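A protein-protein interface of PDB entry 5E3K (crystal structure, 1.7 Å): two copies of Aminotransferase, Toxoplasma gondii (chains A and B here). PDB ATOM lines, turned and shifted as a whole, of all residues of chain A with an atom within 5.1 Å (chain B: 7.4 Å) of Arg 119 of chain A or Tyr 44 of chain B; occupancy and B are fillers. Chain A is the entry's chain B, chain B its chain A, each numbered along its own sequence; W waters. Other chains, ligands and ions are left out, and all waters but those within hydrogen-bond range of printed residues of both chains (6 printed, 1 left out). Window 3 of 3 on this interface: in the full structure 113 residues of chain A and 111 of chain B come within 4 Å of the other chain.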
ATOM      1  N   THR A 114      30.463  -7.840  10.336  1.00  0.00           N
ATOM      2  CA  THR A 114      30.154  -8.135   8.945  1.00  0.00           C
ATOM      3  C   THR A 114      28.759  -7.709   8.539  1.00  0.00           C
ATOM      4  O   THR A 114      28.563  -7.035   7.498  1.00  0.00           O
ATOM      5  CB  THR A 114      30.388  -9.639   8.644  1.00  0.00           C
ATOM      6  OG1 THR A 114      31.766  -9.983   8.899  1.00  0.00           O
ATOM      7  CG2 THR A 114      30.061  -9.957   7.192  1.00  0.00           C
ATOM      8  N   GLY A 115      27.784  -8.067   9.383  1.00  0.00           N
ATOM      9  CA  GLY A 115      26.427  -7.641   9.128  1.00  0.00           C
ATOM     10  C   GLY A 115      26.239  -6.125   9.080  1.00  0.00           C
ATOM     11  O   GLY A 115      25.708  -5.575   8.107  1.00  0.00           O
ATOM     12  N   PRO A 116      26.675  -5.437  10.139  1.00  0.00           N
ATOM     13  CA  PRO A 116      26.551  -3.983  10.111  1.00  0.00           C
ATOM     14  C   PRO A 116      27.231  -3.360   8.881  1.00  0.00           C
ATOM     15  O   PRO A 116      26.695  -2.426   8.295  1.00  0.00           O
ATOM     16  CB  PRO A 116      27.253  -3.551  11.406  1.00  0.00           C
ATOM     17  CG  PRO A 116      26.918  -4.680  12.339  1.00  0.00           C
ATOM     18  CD  PRO A 116      27.022  -5.929  11.484  1.00  0.00           C
ATOM     19  N   ALA A 117      28.373  -3.915   8.470  1.00  0.00           N
ATOM     20  CA  ALA A 117      29.089  -3.374   7.286  1.00  0.00           C
ATOM     21  C   ALA A 117      28.306  -3.593   6.021  1.00  0.00           C
ATOM     22  O   ALA A 117      28.251  -2.714   5.150  1.00  0.00           O
ATOM     23  CB  ALA A 117      30.509  -3.957   7.166  1.00  0.00           C
ATOM     24  N   CYS A 118      27.641  -4.756   5.906  1.00  0.00           N
ATOM     25  CA  CYS A 118      26.832  -5.021   4.752  1.00  0.00           C
ATOM     26  C   CYS A 118      25.599  -4.105   4.749  1.00  0.00           C
ATOM     27  O   CYS A 118      25.256  -3.548   3.701  1.00  0.00           O
ATOM     28  CB  CYS A 118      26.376  -6.481   4.674  1.00  0.00           C
ATOM     29  SG  CYS A 118      27.718  -7.645   4.229  1.00  0.00           S
ATOM     30  N   ARG A 119      25.010  -3.877   5.926  1.00  0.00           N
ATOM     31  CA  ARG A 119      23.879  -2.935   6.031  1.00  0.00           C
ATOM     32  C   ARG A 119      24.354  -1.550   5.603  1.00  0.00           C
ATOM     33  O   ARG A 119      23.708  -0.883   4.823  1.00  0.00           O
ATOM     34  CB  ARG A 119      23.327  -2.832   7.454  1.00  0.00           C
ATOM     35  CG  ARG A 119      22.152  -1.889   7.539  1.00  0.00           C
ATOM     36  CD  ARG A 119      21.474  -1.834   8.916  1.00  0.00           C
ATOM     37  NE  ARG A 119      20.431  -0.826   8.804  1.00  0.00           N
ATOM     38  CZ  ARG A 119      19.289  -0.773   9.475  1.00  0.00           C
ATOM     39  NH1 ARG A 119      18.964  -1.638  10.438  1.00  0.00           N
ATOM     40  NH2 ARG A 119      18.469   0.205   9.157  1.00  0.00           N
ATOM     41  N   PHE A 120      25.537  -1.160   6.074  1.00  0.00           N
ATOM     42  CA  PHE A 120      26.091   0.158   5.676  1.00  0.00           C
ATOM     43  C   PHE A 120      26.188   0.304   4.179  1.00  0.00           C
ATOM     44  O   PHE A 120      25.792   1.318   3.663  1.00  0.00           O
ATOM     45  CB  PHE A 120      27.455   0.347   6.295  1.00  0.00           C
ATOM     46  CG  PHE A 120      28.087   1.670   5.973  1.00  0.00           C
ATOM     47  CD1 PHE A 120      28.828   1.844   4.812  1.00  0.00           C
ATOM     48  CD2 PHE A 120      27.981   2.727   6.862  1.00  0.00           C
ATOM     49  CE1 PHE A 120      29.453   3.079   4.544  1.00  0.00           C
ATOM     50  CE2 PHE A 120      28.603   3.945   6.596  1.00  0.00           C
ATOM     51  CZ  PHE A 120      29.355   4.104   5.462  1.00  0.00           C
ATOM     52  N   MET A 121      26.734  -0.694   3.479  1.00  0.00           N
ATOM     53  CA  MET A 121      26.841  -0.661   2.033  1.00  0.00           C
ATOM     54  C   MET A 121      25.487  -0.778   1.336  1.00  0.00           C
ATOM     55  O   MET A 121      25.281  -0.108   0.340  1.00  0.00           O
ATOM     56  CB  MET A 121      27.768  -1.764   1.533  1.00  0.00           C
ATOM     57  CG  MET A 121      29.171  -1.654   2.105  1.00  0.00           C
ATOM     58  SD  MET A 121      30.250  -2.944   1.404  1.00  0.00           S
ATOM     59  CE  MET A 121      31.571  -2.895   2.585  1.00  0.00           C
ATOM     60  N   ALA A 122      24.589  -1.606   1.866  1.00  0.00           N
ATOM     61  CA  ALA A 122      23.234  -1.763   1.295  1.00  0.00           C
ATOM     62  C   ALA A 122      22.557  -0.414   1.223  1.00  0.00           C
ATOM     63  O   ALA A 122      21.952  -0.110   0.209  1.00  0.00           O
ATOM     64  CB  ALA A 122      22.389  -2.735   2.138  1.00  0.00           C
ATOM     65  N   GLU A 123      22.656   0.360   2.298  1.00  0.00           N
ATOM     66  CA  GLU A 123      21.998   1.661   2.384  1.00  0.00           C
ATOM     67  C   GLU A 123      22.710   2.649   1.507  1.00  0.00           C
ATOM     68  O   GLU A 123      22.079   3.460   0.875  1.00  0.00           O
ATOM     69  CB  GLU A 123      21.927   2.154   3.840  1.00  0.00           C
ATOM     70  CG  GLU A 123      21.004   1.262   4.688  1.00  0.00           C
ATOM     71  CD  GLU A 123      20.905   1.628   6.167  1.00  0.00           C
ATOM     72  OE1 GLU A 123      21.743   2.402   6.696  1.00  0.00           O
ATOM     73  OE2 GLU A 123      19.964   1.091   6.797  1.00  0.00           O
ATOM     74  N   MET A 124      24.039   2.610   1.467  1.00  0.00           N
ATOM     75  CA  MET A 124      24.764   3.604   0.640  1.00  0.00           C
ATOM     76  C   MET A 124      24.487   3.469  -0.846  1.00  0.00           C
ATOM     77  O   MET A 124      24.418   4.490  -1.571  1.00  0.00           O
ATOM     78  CB  MET A 124      26.273   3.530   0.893  1.00  0.00           C
ATOM     79  CG  MET A 124      27.096   4.531   0.109  1.00  0.00           C
ATOM     80  SD  MET A 124      28.814   4.570   0.687  1.00  0.00           S
ATOM     81  CE  MET A 124      28.769   5.711   2.037  1.00  0.00           C
ATOM     82  N   ASP A 128      19.337  -4.593  -1.778  1.00  0.00           N
ATOM     83  CA  ASP A 128      18.833  -5.472  -0.729  1.00  0.00           C
ATOM     84  C   ASP A 128      19.927  -6.312  -0.039  1.00  0.00           C
ATOM     85  O   ASP A 128      19.890  -6.527   1.193  1.00  0.00           O
ATOM     86  CB  ASP A 128      17.792  -6.424  -1.280  1.00  0.00           C
ATOM     87  CG  ASP A 128      16.482  -5.741  -1.742  1.00  0.00           C
ATOM     88  OD1 ASP A 128      16.009  -4.687  -1.219  1.00  0.00           O
ATOM     89  OD2 ASP A 128      15.867  -6.335  -2.621  1.00  0.00           O
ATOM     90  N   ARG A 129      20.811  -6.877  -0.851  1.00  0.00           N
ATOM     91  CA  ARG A 129      21.771  -7.905  -0.369  1.00  0.00           C
ATOM     92  C   ARG A 129      23.154  -7.563  -0.842  1.00  0.00           C
ATOM     93  O   ARG A 129      23.370  -7.209  -1.985  1.00  0.00           O
ATOM     94  CB  ARG A 129      21.463  -9.301  -0.854  1.00  0.00           C
ATOM     95  CG  ARG A 129      20.061  -9.777  -0.601  1.00  0.00           C
ATOM     96  CD  ARG A 129      19.793 -10.179   0.853  1.00  0.00           C
ATOM     97  NE  ARG A 129      18.494 -10.884   0.906  1.00  0.00           N
ATOM     98  CZ  ARG A 129      17.330 -10.458   1.393  1.00  0.00           C
ATOM     99  NH1 ARG A 129      17.170  -9.320   2.074  1.00  0.00           N
ATOM    100  NH2 ARG A 129      16.288 -11.278   1.328  1.00  0.00           N
ATOM    101  N   VAL A 130      24.087  -7.745   0.080  1.00  0.00           N
ATOM    102  CA  VAL A 130      25.526  -7.528  -0.211  1.00  0.00           C
ATOM    103  C   VAL A 130      26.312  -8.826   0.023  1.00  0.00           C
ATOM    104  O   VAL A 130      26.241  -9.432   1.147  1.00  0.00           O
ATOM    105  CB  VAL A 130      26.091  -6.439   0.682  1.00  0.00           C
ATOM    106  CG1 VAL A 130      27.582  -6.249   0.393  1.00  0.00           C
ATOM    107  CG2 VAL A 130      25.336  -5.129   0.466  1.00  0.00           C
ATOM    108  N   TYR B  25      28.752   3.550  13.513  1.00  0.00           N
ATOM    109  CA  TYR B  25      27.630   3.089  12.730  1.00  0.00           C
ATOM    110  C   TYR B  25      26.925   1.963  13.480  1.00  0.00           C
ATOM    111  O   TYR B  25      25.708   2.025  13.689  1.00  0.00           O
ATOM    112  CB  TYR B  25      28.067   2.587  11.353  1.00  0.00           C
ATOM    113  CG  TYR B  25      26.884   2.152  10.529  1.00  0.00           C
ATOM    114  CD1 TYR B  25      25.999   3.087  10.034  1.00  0.00           C
ATOM    115  CD2 TYR B  25      26.657   0.823  10.246  1.00  0.00           C
ATOM    116  CE1 TYR B  25      24.919   2.723   9.253  1.00  0.00           C
ATOM    117  CE2 TYR B  25      25.594   0.433   9.460  1.00  0.00           C
ATOM    118  CZ  TYR B  25      24.709   1.382   8.978  1.00  0.00           C
ATOM    119  OH  TYR B  25      23.651   1.045   8.230  1.00  0.00           O
ATOM    120  N   LEU B  29      22.891   1.354  15.349  1.00  0.00           N
ATOM    121  CA  LEU B  29      21.905   0.306  15.035  1.00  0.00           C
ATOM    122  C   LEU B  29      21.262  -0.319  16.260  1.00  0.00           C
ATOM    123  O   LEU B  29      20.289  -1.069  16.159  1.00  0.00           O
ATOM    124  CB  LEU B  29      22.589  -0.804  14.230  1.00  0.00           C
ATOM    125  CG  LEU B  29      23.247  -0.385  12.921  1.00  0.00           C
ATOM    126  CD1 LEU B  29      23.774  -1.664  12.266  1.00  0.00           C
ATOM    127  CD2 LEU B  29      22.295   0.344  12.018  1.00  0.00           C
ATOM    128  N   LEU B  31      22.059  -2.776  18.327  1.00  0.00           N
ATOM    129  CA  LEU B  31      21.990  -4.225  18.291  1.00  0.00           C
ATOM    130  C   LEU B  31      22.427  -4.729  19.652  1.00  0.00           C
ATOM    131  O   LEU B  31      23.610  -4.554  20.002  1.00  0.00           O
ATOM    132  CB  LEU B  31      22.920  -4.773  17.212  1.00  0.00           C
ATOM    133  CG  LEU B  31      22.640  -4.354  15.764  1.00  0.00           C
ATOM    134  CD1 LEU B  31      23.781  -4.758  14.836  1.00  0.00           C
ATOM    135  CD2 LEU B  31      21.357  -4.988  15.231  1.00  0.00           C
ATOM    136  N   PHE B  38      21.651 -11.721  14.037  1.00  0.00           N
ATOM    137  CA  PHE B  38      21.153 -12.709  13.074  1.00  0.00           C
ATOM    138  C   PHE B  38      20.149 -12.086  12.129  1.00  0.00           C
ATOM    139  O   PHE B  38      20.140 -12.378  10.940  1.00  0.00           O
ATOM    140  CB  PHE B  38      20.512 -13.946  13.746  1.00  0.00           C
ATOM    141  CG  PHE B  38      21.433 -14.729  14.687  1.00  0.00           C
ATOM    142  CD1 PHE B  38      22.834 -14.673  14.592  1.00  0.00           C
ATOM    143  CD2 PHE B  38      20.887 -15.598  15.619  1.00  0.00           C
ATOM    144  CE1 PHE B  38      23.642 -15.393  15.459  1.00  0.00           C
ATOM    145  CE2 PHE B  38      21.692 -16.331  16.480  1.00  0.00           C
ATOM    146  CZ  PHE B  38      23.085 -16.230  16.397  1.00  0.00           C
ATOM    147  N   ALA B  39      19.256 -11.265  12.670  1.00  0.00           N
ATOM    148  CA  ALA B  39      18.285 -10.544  11.847  1.00  0.00           C
ATOM    149  C   ALA B  39      18.952  -9.611  10.827  1.00  0.00           C
ATOM    150  O   ALA B  39      18.525  -9.509   9.639  1.00  0.00           O
ATOM    151  CB  ALA B  39      17.313  -9.779  12.777  1.00  0.00           C
ATOM    152  N   CYS B  40      19.992  -8.913  11.273  1.00  0.00           N
ATOM    153  CA  CYS B  40      20.796  -8.067  10.382  1.00  0.00           C
ATOM    154  C   CYS B  40      21.408  -8.862   9.220  1.00  0.00           C
ATOM    155  O   CYS B  40      21.277  -8.437   8.068  1.00  0.00           O
ATOM    156  CB  CYS B  40      21.796  -7.272  11.196  1.00  0.00           C
ATOM    157  SG  CYS B  40      22.876  -6.155  10.220  1.00  0.00           S
ATOM    158  N   ASP B  41      21.882 -10.108   9.458  1.00  0.00           N
ATOM    159  CA  ASP B  41      22.291 -11.026   8.321  1.00  0.00           C
ATOM    160  C   ASP B  41      21.183 -11.330   7.363  1.00  0.00           C
ATOM    161  O   ASP B  41      21.360 -11.210   6.150  1.00  0.00           O
ATOM    162  CB  ASP B  41      22.779 -12.412   8.806  1.00  0.00           C
ATOM    163  CG  ASP B  41      24.068 -12.342   9.639  1.00  0.00           C
ATOM    164  OD1 ASP B  41      24.811 -11.358   9.494  1.00  0.00           O
ATOM    165  OD2 ASP B  41      24.344 -13.334  10.394  1.00  0.00           O
ATOM    166  N   ARG B  42      20.025 -11.777   7.883  1.00  0.00           N
ATOM    167  CA  ARG B  42      18.957 -12.145   6.977  1.00  0.00           C
ATOM    168  C   ARG B  42      18.548 -10.974   6.107  1.00  0.00           C
ATOM    169  O   ARG B  42      18.104 -11.163   4.949  1.00  0.00           O
ATOM    170  CB  ARG B  42      17.715 -12.661   7.703  1.00  0.00           C
ATOM    171  CG  ARG B  42      17.911 -13.965   8.449  1.00  0.00           C
ATOM    172  CD  ARG B  42      16.550 -14.502   8.911  1.00  0.00           C
ATOM    173  NE  ARG B  42      16.066 -13.721  10.054  1.00  0.00           N
ATOM    174  CZ  ARG B  42      16.461 -13.919  11.323  1.00  0.00           C
ATOM    175  NH1 ARG B  42      17.328 -14.860  11.626  1.00  0.00           N
ATOM    176  NH2 ARG B  42      15.958 -13.187  12.309  1.00  0.00           N
ATOM    177  N   GLN B  43      18.609  -9.760   6.658  1.00  0.00           N
ATOM    178  CA  GLN B  43      18.138  -8.622   5.878  1.00  0.00           C
ATOM    179  C   GLN B  43      19.151  -8.134   4.881  1.00  0.00           C
ATOM    180  O   GLN B  43      18.769  -7.763   3.786  1.00  0.00           O
ATOM    181  CB  GLN B  43      17.686  -7.457   6.773  1.00  0.00           C
ATOM    182  CG  GLN B  43      17.045  -6.263   6.028  1.00  0.00           C
ATOM    183  CD  GLN B  43      15.680  -6.554   5.298  1.00  0.00           C
ATOM    184  OE1 GLN B  43      15.512  -6.330   4.079  1.00  0.00           O
ATOM    185  NE2 GLN B  43      14.720  -6.998   6.043  1.00  0.00           N
ATOM    186  N   TYR B  44      20.435  -8.069   5.246  1.00  0.00           N
ATOM    187  CA  TYR B  44      21.416  -7.337   4.406  1.00  0.00           C
ATOM    188  C   TYR B  44      22.579  -8.160   3.799  1.00  0.00           C
ATOM    189  O   TYR B  44      23.233  -7.699   2.867  1.00  0.00           O
ATOM    190  CB  TYR B  44      22.024  -6.179   5.190  1.00  0.00           C
ATOM    191  CG  TYR B  44      20.971  -5.218   5.669  1.00  0.00           C
ATOM    192  CD1 TYR B  44      20.347  -4.342   4.790  1.00  0.00           C
ATOM    193  CD2 TYR B  44      20.578  -5.201   6.982  1.00  0.00           C
ATOM    194  CE1 TYR B  44      19.384  -3.454   5.212  1.00  0.00           C
ATOM    195  CE2 TYR B  44      19.602  -4.338   7.404  1.00  0.00           C
ATOM    196  CZ  TYR B  44      19.033  -3.464   6.513  1.00  0.00           C
ATOM    197  OH  TYR B  44      18.026  -2.619   6.978  1.00  0.00           O
ATOM    198  N   VAL B  45      22.790  -9.373   4.292  1.00  0.00           N
ATOM    199  CA  VAL B  45      23.982 -10.167   3.901  1.00  0.00           C
ATOM    200  C   VAL B  45      23.497 -11.258   2.971  1.00  0.00           C
ATOM    201  O   VAL B  45      22.505 -11.963   3.264  1.00  0.00           O
ATOM    202  CB  VAL B  45      24.684 -10.779   5.100  1.00  0.00           C
ATOM    203  CG1 VAL B  45      25.904 -11.596   4.673  1.00  0.00           C
ATOM    204  CG2 VAL B  45      25.079  -9.698   6.105  1.00  0.00           C
ATOM    205  N   CYS B  46      24.126 -11.342   1.818  1.00  0.00           N
ATOM    206  CA  CYS B  46      23.841 -12.447   0.867  1.00  0.00           C
ATOM    207  C   CYS B  46      23.785 -13.742   1.623  1.00  0.00           C
ATOM    208  O   CYS B  46      24.713 -14.044   2.365  1.00  0.00           O
ATOM    209  CB  CYS B  46      24.949 -12.480  -0.189  1.00  0.00           C
ATOM    210  SG  CYS B  46      24.654 -13.695  -1.516  1.00  0.00           S
ATOM    211  N   GLN B  47      22.695 -14.504   1.495  1.00  0.00           N
ATOM    212  CA  GLN B  47      22.395 -15.616   2.410  1.00  0.00           C
ATOM    213  C   GLN B  47      23.008 -16.987   2.011  1.00  0.00           C
ATOM    214  O   GLN B  47      22.358 -18.041   2.110  1.00  0.00           O
ATOM    215  CB  GLN B  47      20.883 -15.771   2.559  1.00  0.00           C
ATOM    216  CG  GLN B  47      20.173 -16.151   1.260  1.00  0.00           C
ATOM    217  CD  GLN B  47      18.835 -16.880   1.412  1.00  0.00           C
ATOM    218  OE1 GLN B  47      18.389 -17.114   2.507  1.00  0.00           O
ATOM    219  NE2 GLN B  47      18.196 -17.235   0.301  1.00  0.00           N
HETATM  220  O   HOH W   1      15.239 -10.615   4.371  1.00  0.00           O
HETATM  221  O   HOH W   2      17.658  -5.084   2.830  1.00  0.00           O
HETATM  222  O   HOH W   3      20.458  -3.627  11.583  1.00  0.00           O
HETATM  223  O   HOH W   4      17.996  -0.170   5.828  1.00  0.00           O
HETATM  224  O   HOH W   5      17.778 -14.266   2.111  1.00  0.00           O
HETATM  225  O   HOH W   6      19.382  -2.012  13.848  1.00  0.00           O
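O of Thr 114 of chain A sits at hydrogen-bond distance from SG of Cys 118 of chain A (3.4 Å). OE2 of Glu 123 of chain A is in salt-bridge range of NE of Arg 119 of chain A, 2.8 Å away.
Of the 14 printed residues of chain A, 10 touch a printed residue of chain B. Hydrophobic or aromatic side chains of chain A within 4 Å of the printed part of chain B: Phe 120, Ala 122 and Val 130. Hydrophobic or aromatic side chains of chain B that line the printed part of chain A: Tyr 25, Leu 29, Tyr 44 and Val 45.
Among the printed residues, pairs that only touch across the chains: Pro 116 of chain A with Tyr 25 of chain B (3.3 Å), Arg 119 of chain A with Tyr 44 of chain B (3.4 Å), Arg 119 of chain A with Tyr 25 of chain B (3.4 Å), Arg 129 of chain A with Arg 42 of chain B (3.5 Å), Arg 129 of chain A with Tyr 44 of chain B (3.6 Å), Phe 120 of chain A with Tyr 25 of chain B (3.6 Å), Val 130 of chain A with Val 45 of chain B (3.6 Å), Asp 128 of chain A with Tyr 44 of chain B (3.6 Å), Ala 122 of chain A with Tyr 44 of chain B (3.7 Å), Cys 118 of chain A with Val 45 of chain B (3.8 Å), Cys 118 of chain A with Tyr 44 of chain B (3.8 Å), Pro 116 of chain A with Cys 40 of chain B (3.9 Å), Arg 119 of chain A with Leu 29 of chain B (3.9 Å) and Gly 115 of chain A with Val 45 of chain B (3.9 Å).
Water W4 lies within hydrogen-bond range of OE2 of Glu 123 of chain A (2.5 Å), OH of Tyr 44 of chain B (2.7 Å) and NH2 of Arg 119 of chain A (3.4 Å). Water W6 bridges the backbone carbonyl oxygen of Leu 29 of chain B (2.7 Å) and the guanidinium group of Arg 119 of chain A (3.5 Å). Water W3 bridges the guanidinium group (NH1) of Arg 119 of chain A (2.7 Å) and the side-chain sulfur (SG) of Cys 40 of chain B (3.8 Å). Water W2 lies within hydrogen-bond range of OE1 of Gln 43 of chain B (2.8 Å) and O of Asp 128 of chain A (3.1 Å). Water W5 lies within hydrogen-bond range of OE1 of Gln 47 of chain B (2.9 Å) and NH2 of Arg 129 of chain A (3.4 Å). Water W1 lies within hydrogen-bond range of O of Arg 42 of chain B (3.0 Å) and NH1 of Arg 129 of chain A (3.3 Å).
No position is printed for both chains.
Arg 119 of chain A touches three residues of chain B. Printed residues of chain A within 4 Å of Tyr 44 of chain B: Cys 118 (3.8 Å), Arg 119 (3.4 Å), Ala 122 (3.7 Å), Asp 128 (3.6 Å), Arg 129 (3.6 Å) and Val 130 (2.9 Å). Of the printed residues of chain A, Cys 46 of chain B touches Val 130. Of the printed residues of chain B, Arg 129 of chain A touches Arg 42, Gln 43 and Tyr 44. Printed residues of chain A within 4 Å of Leu 29 of chain B: Arg 119 (3.9 Å). Of the printed residues of chain B, Cys 118 of chain A touches Tyr 44 (3.8 Å) and Val 45 (3.8 Å). Printed residues of chain B within 4 Å of Gly 115 of chain A: Cys 40 (3.6 Å) and Val 45 (3.9 Å). The nearest residue of chain B that does not touch Arg 119 of chain A is Cys 40 of chain B (4.3 Å). The nearest printed residue of chain B that does not touch Pro 116 of chain A is Leu 31 of chain B (4.01 Å).
The side-chain carboxylate (OE1) of Glu 123 of chain A is in hydrogen-bond range of the side-chain hydroxyl (OH) of Tyr 25 of chain B. The side-chain sulfur (SG) of Cys 40 of chain B lies close to the backbone carbonyl oxygen (O) of Gly 115 of chain A (3.6 Å). The backbone carbonyl oxygen of Gln 43 of chain B is in hydrogen-bond range of the guanidinium group of Arg 129 of chain A. The backbone carbonyl oxygen (O) of Tyr 44 of chain B is in hydrogen-bond range of the backbone NH (N) of Val 130 of chain A, 2.9 Å away. O of Val 130 of chain A sits at hydrogen-bond distance from N of Cys 46 of chain B. The backbone carbonyl oxygen (O) of Asp 128 of chain A sits close to the backbone carbonyl oxygen (O) of Gln 43 of chain B.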
